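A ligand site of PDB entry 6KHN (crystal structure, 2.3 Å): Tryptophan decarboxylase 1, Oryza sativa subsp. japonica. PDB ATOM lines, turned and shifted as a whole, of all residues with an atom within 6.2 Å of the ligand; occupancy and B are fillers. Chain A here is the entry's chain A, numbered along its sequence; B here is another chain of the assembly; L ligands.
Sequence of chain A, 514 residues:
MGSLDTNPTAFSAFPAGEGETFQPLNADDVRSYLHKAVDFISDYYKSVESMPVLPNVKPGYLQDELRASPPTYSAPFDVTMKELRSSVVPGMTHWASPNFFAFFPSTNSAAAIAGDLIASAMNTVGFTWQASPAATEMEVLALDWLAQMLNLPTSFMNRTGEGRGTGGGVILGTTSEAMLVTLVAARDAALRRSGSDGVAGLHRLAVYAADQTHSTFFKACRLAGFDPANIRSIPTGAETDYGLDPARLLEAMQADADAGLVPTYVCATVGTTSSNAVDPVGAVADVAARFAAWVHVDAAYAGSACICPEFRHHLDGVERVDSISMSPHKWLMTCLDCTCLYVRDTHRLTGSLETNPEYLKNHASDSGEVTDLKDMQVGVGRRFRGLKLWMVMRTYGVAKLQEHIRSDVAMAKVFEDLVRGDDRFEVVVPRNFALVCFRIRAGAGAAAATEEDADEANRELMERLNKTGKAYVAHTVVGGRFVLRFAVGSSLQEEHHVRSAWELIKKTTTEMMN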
ATOM      1  N   PHE A 104      14.031  15.810  -5.362  1.00  0.00           N
ATOM      2  CA  PHE A 104      13.845  14.382  -5.474  1.00  0.00           C
ATOM      3  C   PHE A 104      15.097  13.777  -6.078  1.00  0.00           C
ATOM      4  O   PHE A 104      15.711  14.385  -6.950  1.00  0.00           O
ATOM      5  CB  PHE A 104      12.624  14.057  -6.351  1.00  0.00           C
ATOM      6  CG  PHE A 104      11.326  14.490  -5.746  1.00  0.00           C
ATOM      7  CD1 PHE A 104      10.837  13.855  -4.597  1.00  0.00           C
ATOM      8  CD2 PHE A 104      10.609  15.538  -6.290  1.00  0.00           C
ATOM      9  CE1 PHE A 104       9.628  14.257  -4.029  1.00  0.00           C
ATOM     10  CE2 PHE A 104       9.399  15.939  -5.722  1.00  0.00           C
ATOM     11  CZ  PHE A 104       8.916  15.301  -4.589  1.00  0.00           C
ATOM     12  N   GLY A 173      11.508  15.795 -22.854  1.00  0.00           N
ATOM     13  CA  GLY A 173      12.580  16.090 -21.928  1.00  0.00           C
ATOM     14  C   GLY A 173      12.128  16.420 -20.516  1.00  0.00           C
ATOM     15  O   GLY A 173      12.773  16.020 -19.555  1.00  0.00           O
ATOM     16  N   THR A 174      11.009  17.150 -20.375  1.00  0.00           N
ATOM     17  CA  THR A 174      10.655  17.745 -19.095  1.00  0.00           C
ATOM     18  C   THR A 174       9.152  17.708 -18.910  1.00  0.00           C
ATOM     19  O   THR A 174       8.383  17.693 -19.862  1.00  0.00           O
ATOM     20  CB  THR A 174      11.118  19.208 -19.000  1.00  0.00           C
ATOM     21  OG1 THR A 174      10.515  19.969 -20.055  1.00  0.00           O
ATOM     22  CG2 THR A 174      12.655  19.332 -19.075  1.00  0.00           C
ATOM     23  N   THR A 175       8.737  17.732 -17.641  1.00  0.00           N
ATOM     24  CA  THR A 175       7.340  17.945 -17.318  1.00  0.00           C
ATOM     25  C   THR A 175       6.854  19.298 -17.857  1.00  0.00           C
ATOM     26  O   THR A 175       5.713  19.426 -18.315  1.00  0.00           O
ATOM     27  CB  THR A 175       7.140  17.851 -15.806  1.00  0.00           C
ATOM     28  OG1 THR A 175       7.313  16.480 -15.417  1.00  0.00           O
ATOM     29  CG2 THR A 175       5.732  18.289 -15.392  1.00  0.00           C
ATOM     30  N   SER A 176       7.724  20.316 -17.842  1.00  0.00           N
ATOM     31  CA  SER A 176       7.343  21.617 -18.369  1.00  0.00           C
ATOM     32  C   SER A 176       6.867  21.511 -19.811  1.00  0.00           C
ATOM     33  O   SER A 176       5.868  22.138 -20.187  1.00  0.00           O
ATOM     34  CB  SER A 176       8.517  22.592 -18.293  1.00  0.00           C
ATOM     35  OG  SER A 176       8.947  22.771 -16.960  1.00  0.00           O
ATOM     36  N   GLU A 177       7.579  20.762 -20.657  1.00  0.00           N
ATOM     37  CA  GLU A 177       7.141  20.630 -22.042  1.00  0.00           C
ATOM     38  C   GLU A 177       5.823  19.869 -22.115  1.00  0.00           C
ATOM     39  O   GLU A 177       4.977  20.197 -22.959  1.00  0.00           O
ATOM     40  CB  GLU A 177       8.219  19.944 -22.894  1.00  0.00           C
ATOM     41  CG  GLU A 177       7.906  20.043 -24.386  1.00  0.00           C
ATOM     42  CD  GLU A 177       9.002  19.514 -25.290  1.00  0.00           C
ATOM     43  OE1 GLU A 177      10.053  19.041 -24.777  1.00  0.00           O
ATOM     44  OE2 GLU A 177       8.794  19.545 -26.527  1.00  0.00           O
ATOM     45  N   MET A 179       3.430  19.858 -19.823  1.00  0.00           N
ATOM     46  CA  MET A 179       2.409  20.833 -19.482  1.00  0.00           C
ATOM     47  C   MET A 179       2.178  21.807 -20.629  1.00  0.00           C
ATOM     48  O   MET A 179       1.028  22.136 -20.952  1.00  0.00           O
ATOM     49  CB  MET A 179       2.816  21.582 -18.218  1.00  0.00           C
ATOM     50  CG  MET A 179       2.676  20.724 -16.972  1.00  0.00           C
ATOM     51  SD  MET A 179       3.566  21.479 -15.602  1.00  0.00           S
ATOM     52  CE  MET A 179       3.040  20.417 -14.247  1.00  0.00           C
ATOM     53  N   HIS A 214       3.687  22.504  -8.962  1.00  0.00           N
ATOM     54  CA  HIS A 214       5.049  22.964  -9.232  1.00  0.00           C
ATOM     55  C   HIS A 214       5.034  24.260 -10.025  1.00  0.00           C
ATOM     56  O   HIS A 214       4.197  24.452 -10.914  1.00  0.00           O
ATOM     57  CB  HIS A 214       5.835  21.885  -9.995  1.00  0.00           C
ATOM     58  CG  HIS A 214       7.315  22.148 -10.049  1.00  0.00           C
ATOM     59  ND1 HIS A 214       7.861  23.174 -10.791  1.00  0.00           N
ATOM     60  CD2 HIS A 214       8.352  21.511  -9.463  1.00  0.00           C
ATOM     61  CE1 HIS A 214       9.182  23.147 -10.659  1.00  0.00           C
ATOM     62  NE2 HIS A 214       9.505  22.149  -9.851  1.00  0.00           N
ATOM     63  N   THR A 216       6.709  25.383 -12.374  1.00  0.00           N
ATOM     64  CA  THR A 216       6.815  25.276 -13.819  1.00  0.00           C
ATOM     65  C   THR A 216       5.441  25.224 -14.504  1.00  0.00           C
ATOM     66  O   THR A 216       5.313  25.637 -15.663  1.00  0.00           O
ATOM     67  CB  THR A 216       7.692  24.072 -14.179  1.00  0.00           C
ATOM     68  OG1 THR A 216       8.298  24.297 -15.449  1.00  0.00           O
ATOM     69  CG2 THR A 216       6.885  22.759 -14.199  1.00  0.00           C
ATOM     70  N   THR A 269      -2.061  17.412  -9.359  1.00  0.00           N
ATOM     71  CA  THR A 269      -0.764  16.821  -9.051  1.00  0.00           C
ATOM     72  C   THR A 269      -0.939  15.642  -8.091  1.00  0.00           C
ATOM     73  O   THR A 269      -1.630  15.747  -7.083  1.00  0.00           O
ATOM     74  CB  THR A 269       0.196  17.863  -8.439  1.00  0.00           C
ATOM     75  OG1 THR A 269       0.424  18.918  -9.369  1.00  0.00           O
ATOM     76  CG2 THR A 269       1.557  17.225  -8.115  1.00  0.00           C
ATOM     77  N   VAL A 270      -0.271  14.535  -8.416  1.00  0.00           N
ATOM     78  CA  VAL A 270      -0.136  13.372  -7.539  1.00  0.00           C
ATOM     79  C   VAL A 270       1.322  13.297  -7.096  1.00  0.00           C
ATOM     80  O   VAL A 270       2.201  12.903  -7.870  1.00  0.00           O
ATOM     81  CB  VAL A 270      -0.563  12.085  -8.249  1.00  0.00           C
ATOM     82  CG1 VAL A 270      -0.305  10.871  -7.372  1.00  0.00           C
ATOM     83  CG2 VAL A 270      -2.043  12.176  -8.629  1.00  0.00           C
ATOM     84  N   GLY A 271       1.585  13.691  -5.850  1.00  0.00           N
ATOM     85  CA  GLY A 271       2.951  13.743  -5.332  1.00  0.00           C
ATOM     86  C   GLY A 271       3.587  15.102  -5.496  1.00  0.00           C
ATOM     87  O   GLY A 271       4.518  15.264  -6.284  1.00  0.00           O
ATOM     88  N   THR A 272       3.093  16.099  -4.755  1.00  0.00           N
ATOM     89  CA  THR A 272       3.543  17.461  -4.973  1.00  0.00           C
ATOM     90  C   THR A 272       5.007  17.601  -4.575  1.00  0.00           C
ATOM     91  O   THR A 272       5.539  16.840  -3.765  1.00  0.00           O
ATOM     92  CB  THR A 272       2.696  18.478  -4.198  1.00  0.00           C
ATOM     93  OG1 THR A 272       2.722  18.191  -2.785  1.00  0.00           O
ATOM     94  CG2 THR A 272       1.244  18.513  -4.699  1.00  0.00           C
ATOM     95  N   THR A 273       5.648  18.606  -5.165  1.00  0.00           N
ATOM     96  CA  THR A 273       7.078  18.770  -4.979  1.00  0.00           C
ATOM     97  C   THR A 273       7.418  19.075  -3.521  1.00  0.00           C
ATOM     98  O   THR A 273       8.372  18.533  -2.963  1.00  0.00           O
ATOM     99  CB  THR A 273       7.602  19.854  -5.932  1.00  0.00           C
ATOM    100  OG1 THR A 273       8.967  20.135  -5.641  1.00  0.00           O
ATOM    101  CG2 THR A 273       6.814  21.145  -5.770  1.00  0.00           C
ATOM    102  N   ASP A 298      -0.176  15.691 -13.235  1.00  0.00           N
ATOM    103  CA  ASP A 298       1.262  15.743 -13.087  1.00  0.00           C
ATOM    104  C   ASP A 298       1.671  14.761 -11.995  1.00  0.00           C
ATOM    105  O   ASP A 298       1.468  15.030 -10.807  1.00  0.00           O
ATOM    106  CB  ASP A 298       1.739  17.156 -12.737  1.00  0.00           C
ATOM    107  CG  ASP A 298       3.237  17.199 -12.378  1.00  0.00           C
ATOM    108  OD1 ASP A 298       3.964  16.219 -12.676  1.00  0.00           O
ATOM    109  OD2 ASP A 298       3.684  18.229 -11.810  1.00  0.00           O
ATOM    110  N   ALA A 299       2.250  13.633 -12.391  1.00  0.00           N
ATOM    111  CA  ALA A 299       2.768  12.640 -11.459  1.00  0.00           C
ATOM    112  C   ALA A 299       4.270  12.483 -11.646  1.00  0.00           C
ATOM    113  O   ALA A 299       4.795  11.353 -11.645  1.00  0.00           O
ATOM    114  CB  ALA A 299       2.060  11.313 -11.629  1.00  0.00           C
ATOM    115  N   ALA A 300       4.974  13.609 -11.791  1.00  0.00           N
ATOM    116  CA  ALA A 300       6.379  13.600 -12.181  1.00  0.00           C
ATOM    117  C   ALA A 300       7.196  12.633 -11.339  1.00  0.00           C
ATOM    118  O   ALA A 300       7.905  11.760 -11.859  1.00  0.00           O
ATOM    119  CB  ALA A 300       6.962  15.017 -12.108  1.00  0.00           C
ATOM    120  N   TYR A 301       7.087  12.760 -10.019  1.00  0.00           N
ATOM    121  CA  TYR A 301       7.843  11.935  -9.089  1.00  0.00           C
ATOM    122  C   TYR A 301       7.100  10.641  -8.746  1.00  0.00           C
ATOM    123  O   TYR A 301       7.603   9.539  -9.006  1.00  0.00           O
ATOM    124  CB  TYR A 301       8.130  12.735  -7.811  1.00  0.00           C
ATOM    125  CG  TYR A 301       8.558  11.903  -6.623  1.00  0.00           C
ATOM    126  CD1 TYR A 301       9.811  11.292  -6.603  1.00  0.00           C
ATOM    127  CD2 TYR A 301       7.726  11.742  -5.524  1.00  0.00           C
ATOM    128  CE1 TYR A 301      10.228  10.537  -5.520  1.00  0.00           C
ATOM    129  CE2 TYR A 301       8.134  10.984  -4.432  1.00  0.00           C
ATOM    130  CZ  TYR A 301       9.387  10.391  -4.434  1.00  0.00           C
ATOM    131  OH  TYR A 301       9.800   9.629  -3.358  1.00  0.00           O
ATOM    132  N   SER A 327       7.856  11.172 -14.785  1.00  0.00           N
ATOM    133  CA  SER A 327       9.258  11.241 -15.202  1.00  0.00           C
ATOM    134  C   SER A 327      10.039  10.044 -14.686  1.00  0.00           C
ATOM    135  O   SER A 327      10.393  10.001 -13.495  1.00  0.00           O
ATOM    136  CB  SER A 327       9.900  12.542 -14.734  1.00  0.00           C
ATOM    137  OG  SER A 327       9.254  13.650 -15.331  1.00  0.00           O
ATOM    138  N   HIS A 329      13.021   9.790 -15.102  1.00  0.00           N
ATOM    139  CA  HIS A 329      14.282  10.349 -14.640  1.00  0.00           C
ATOM    140  C   HIS A 329      14.228  10.855 -13.207  1.00  0.00           C
ATOM    141  O   HIS A 329      15.223  11.407 -12.717  1.00  0.00           O
ATOM    142  CB  HIS A 329      14.810  11.440 -15.587  1.00  0.00           C
ATOM    143  CG  HIS A 329      14.052  12.725 -15.557  1.00  0.00           C
ATOM    144  ND1 HIS A 329      13.736  13.417 -16.714  1.00  0.00           N
ATOM    145  CD2 HIS A 329      13.580  13.487 -14.542  1.00  0.00           C
ATOM    146  CE1 HIS A 329      13.096  14.527 -16.411  1.00  0.00           C
ATOM    147  NE2 HIS A 329      12.990  14.601 -15.096  1.00  0.00           N
ATOM    148  N   LYS A 330      13.111  10.696 -12.523  1.00  0.00           N
ATOM    149  CA  LYS A 330      13.142  10.932 -11.087  1.00  0.00           C
ATOM    150  C   LYS A 330      13.295   9.597 -10.387  1.00  0.00           C
ATOM    151  O   LYS A 330      14.376   9.261  -9.891  1.00  0.00           O
ATOM    152  CB  LYS A 330      11.899  11.701 -10.622  1.00  0.00           C
ATOM    153  CG  LYS A 330      11.992  13.204 -10.900  1.00  0.00           C
ATOM    154  CD  LYS A 330      10.785  13.964 -10.363  1.00  0.00           C
ATOM    155  CE  LYS A 330      10.683  15.334 -11.035  1.00  0.00           C
ATOM    156  NZ  LYS A 330      10.965  16.485 -10.116  1.00  0.00           N
ATOM    157  N   THR A 339      10.810  12.142 -19.646  1.00  0.00           N
ATOM    158  CA  THR A 339       9.479  12.402 -19.116  1.00  0.00           C
ATOM    159  C   THR A 339       8.479  11.810 -20.100  1.00  0.00           C
ATOM    160  O   THR A 339       8.598  12.017 -21.304  1.00  0.00           O
ATOM    161  CB  THR A 339       9.254  13.903 -18.927  1.00  0.00           C
ATOM    162  OG1 THR A 339      10.099  14.378 -17.887  1.00  0.00           O
ATOM    163  CG2 THR A 339       7.823  14.207 -18.557  1.00  0.00           C
ATOM    164  N   VAL B 125      21.101  17.889 -11.815  1.00  0.00           N
ATOM    165  CA  VAL B 125      20.038  18.771 -12.308  1.00  0.00           C
ATOM    166  C   VAL B 125      20.425  20.191 -11.941  1.00  0.00           C
ATOM    167  O   VAL B 125      20.465  20.544 -10.757  1.00  0.00           O
ATOM    168  CB  VAL B 125      18.667  18.404 -11.719  1.00  0.00           C
ATOM    169  CG1 VAL B 125      17.535  19.004 -12.555  1.00  0.00           C
ATOM    170  CG2 VAL B 125      18.538  16.886 -11.569  1.00  0.00           C
ATOM    171  N   VAL B 378      12.141  26.189 -21.797  1.00  0.00           N
ATOM    172  CA  VAL B 378      10.828  25.628 -21.504  1.00  0.00           C
ATOM    173  C   VAL B 378      10.803  25.083 -20.082  1.00  0.00           C
ATOM    174  O   VAL B 378       9.949  25.466 -19.277  1.00  0.00           O
ATOM    175  CB  VAL B 378      10.455  24.565 -22.559  1.00  0.00           C
ATOM    176  CG1 VAL B 378       9.270  23.733 -22.083  1.00  0.00           C
ATOM    177  CG2 VAL B 378      10.137  25.235 -23.875  1.00  0.00           C
ATOM    178  N   GLY B 379      11.748  24.221 -19.742  1.00  0.00           N
ATOM    179  CA  GLY B 379      11.762  23.515 -18.474  1.00  0.00           C
ATOM    180  C   GLY B 379      12.920  23.893 -17.570  1.00  0.00           C
ATOM    181  O   GLY B 379      14.061  24.013 -18.016  1.00  0.00           O
ATOM    182  N   VAL B 380      12.614  24.030 -16.272  1.00  0.00           N
ATOM    183  CA  VAL B 380      13.594  24.507 -15.304  1.00  0.00           C
ATOM    184  C   VAL B 380      14.795  23.569 -15.227  1.00  0.00           C
ATOM    185  O   VAL B 380      15.956  24.009 -15.273  1.00  0.00           O
ATOM    186  CB  VAL B 380      12.911  24.728 -13.933  1.00  0.00           C
ATOM    187  CG1 VAL B 380      11.548  25.423 -14.120  1.00  0.00           C
ATOM    188  CG2 VAL B 380      12.728  23.422 -13.101  1.00  0.00           C
ATOM    189  N   GLY B 381      14.549  22.258 -15.169  1.00  0.00           N
ATOM    190  CA  GLY B 381      15.582  21.321 -14.812  1.00  0.00           C
ATOM    191  C   GLY B 381      15.783  20.235 -15.835  1.00  0.00           C
ATOM    192  O   GLY B 381      14.898  19.385 -16.048  1.00  0.00           O
ATOM    193  N   ARG B 382      16.945  20.232 -16.469  1.00  0.00           N
ATOM    194  CA  ARG B 382      17.315  19.236 -17.456  1.00  0.00           C
ATOM    195  C   ARG B 382      18.803  18.927 -17.276  1.00  0.00           C
ATOM    196  O   ARG B 382      19.475  19.483 -16.393  1.00  0.00           O
ATOM    197  CB  ARG B 382      16.961  19.708 -18.867  1.00  0.00           C
ATOM    198  CG  ARG B 382      17.197  21.208 -19.132  1.00  0.00           C
ATOM    199  CD  ARG B 382      18.685  21.527 -19.140  1.00  0.00           C
ATOM    200  NE  ARG B 382      18.977  22.914 -19.508  1.00  0.00           N
ATOM    201  CZ  ARG B 382      20.206  23.380 -19.751  1.00  0.00           C
ATOM    202  NH1 ARG B 382      21.254  22.568 -19.677  1.00  0.00           N
ATOM    203  NH2 ARG B 382      20.375  24.659 -20.079  1.00  0.00           N
HETATM  204  N1  LIG L   1       6.285  18.402 -11.183  1.00  0.00           N
HETATM  205  C1  LIG L   1       6.504  17.721  -9.994  1.00  0.00           C
HETATM  206  C2  LIG L   1       5.372  17.160  -9.184  1.00  0.00           C
HETATM  207  C3  LIG L   1       7.808  17.560  -9.533  1.00  0.00           C
HETATM  208  O1  LIG L   1       7.960  16.882  -8.355  1.00  0.00           O
HETATM  209  C4  LIG L   1       8.902  18.070 -10.255  1.00  0.00           C
HETATM  210  C5  LIG L   1      10.330  17.738  -9.853  1.00  0.00           C
HETATM  211  C6  LIG L   1       8.685  18.734 -11.459  1.00  0.00           C
HETATM  212  C7  LIG L   1       7.362  18.895 -11.907  1.00  0.00           C
HETATM  213  C8  LIG L   1       9.866  19.298 -12.252  1.00  0.00           C
HETATM  214  O2  LIG L   1       9.562  19.349 -13.642  1.00  0.00           O
HETATM  215  P1  LIG L   1      10.701  19.477 -14.813  1.00  0.00           P
HETATM  216  O3  LIG L   1      11.954  20.017 -14.136  1.00  0.00           O
HETATM  217  O4  LIG L   1      10.974  18.116 -15.478  1.00  0.00           O
HETATM  218  O5  LIG L   1      10.250  20.457 -15.894  1.00  0.00           O
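An oxygen (O5) of the ligand sits at hydrogen-bond distance from the backbone NH (N) of Ser 176 (3.2 Å). The backbone NH of Thr 175 is in hydrogen-bond range of an oxygen (O4) of the ligand, 3.1 Å away. An oxygen (O5) of the ligand sits at hydrogen-bond distance from the side-chain hydroxyl (OG) of Ser 176 (2.9 Å). C5 of the ligand is bonded to NZ of Lys 330 (1.4 Å). A nitrogen (N1) of the ligand sits at hydrogen-bond distance from the side-chain carboxylate (OD2) of Asp 298, at 2.7 Å.
The side-chain carboxylate of Asp 298 lies within hydrogen-bond range of the backbone NH of Ala 300 (2.9 Å). The backbone NH (N) of Glu 177 is in hydrogen-bond range of the side-chain hydroxyl (OG1) of Thr 174 (3.1 Å). The side-chain hydroxyl (OG1) of Thr 175 is in hydrogen-bond range of the side-chain hydroxyl (OG) of Ser 327 (3.4 Å). A ring nitrogen (ND1) of His 214 is in hydrogen-bond range of the backbone NH (N) of Thr 216, 3.0 Å away. N of Val 270 is in hydrogen-bond range of O of Asp 298. The backbone carbonyl oxygen (O) of Ala 300 lies within hydrogen-bond range of the backbone NH (N) of Ser 327 (3.0 Å).
Phe 104 touches the ligand (CE2 to O1, 3.1 Å). Thr 174 touches the ligand (CB to O5, 3.5 Å). His 214 touches the ligand (CD2 to C6, 3.4 Å). Thr 269 touches the ligand. O of Gly 271 touches C2 of the ligand, at 3.6 Å. Thr 273 touches the ligand. Ala 300 touches the ligand (CB to C1, 3.5 Å). Val 380 of chain B touches the ligand. Gly 381 of chain B touches the ligand (O to O3, 3.6 Å). Hydrophobic or aromatic side chains within 4 Å of the ligand: Phe 104, His 214, Ala 300 and Val 380 of chain B. The nearest printed residue that does not touch the ligand is His 329 (4.1 Å).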
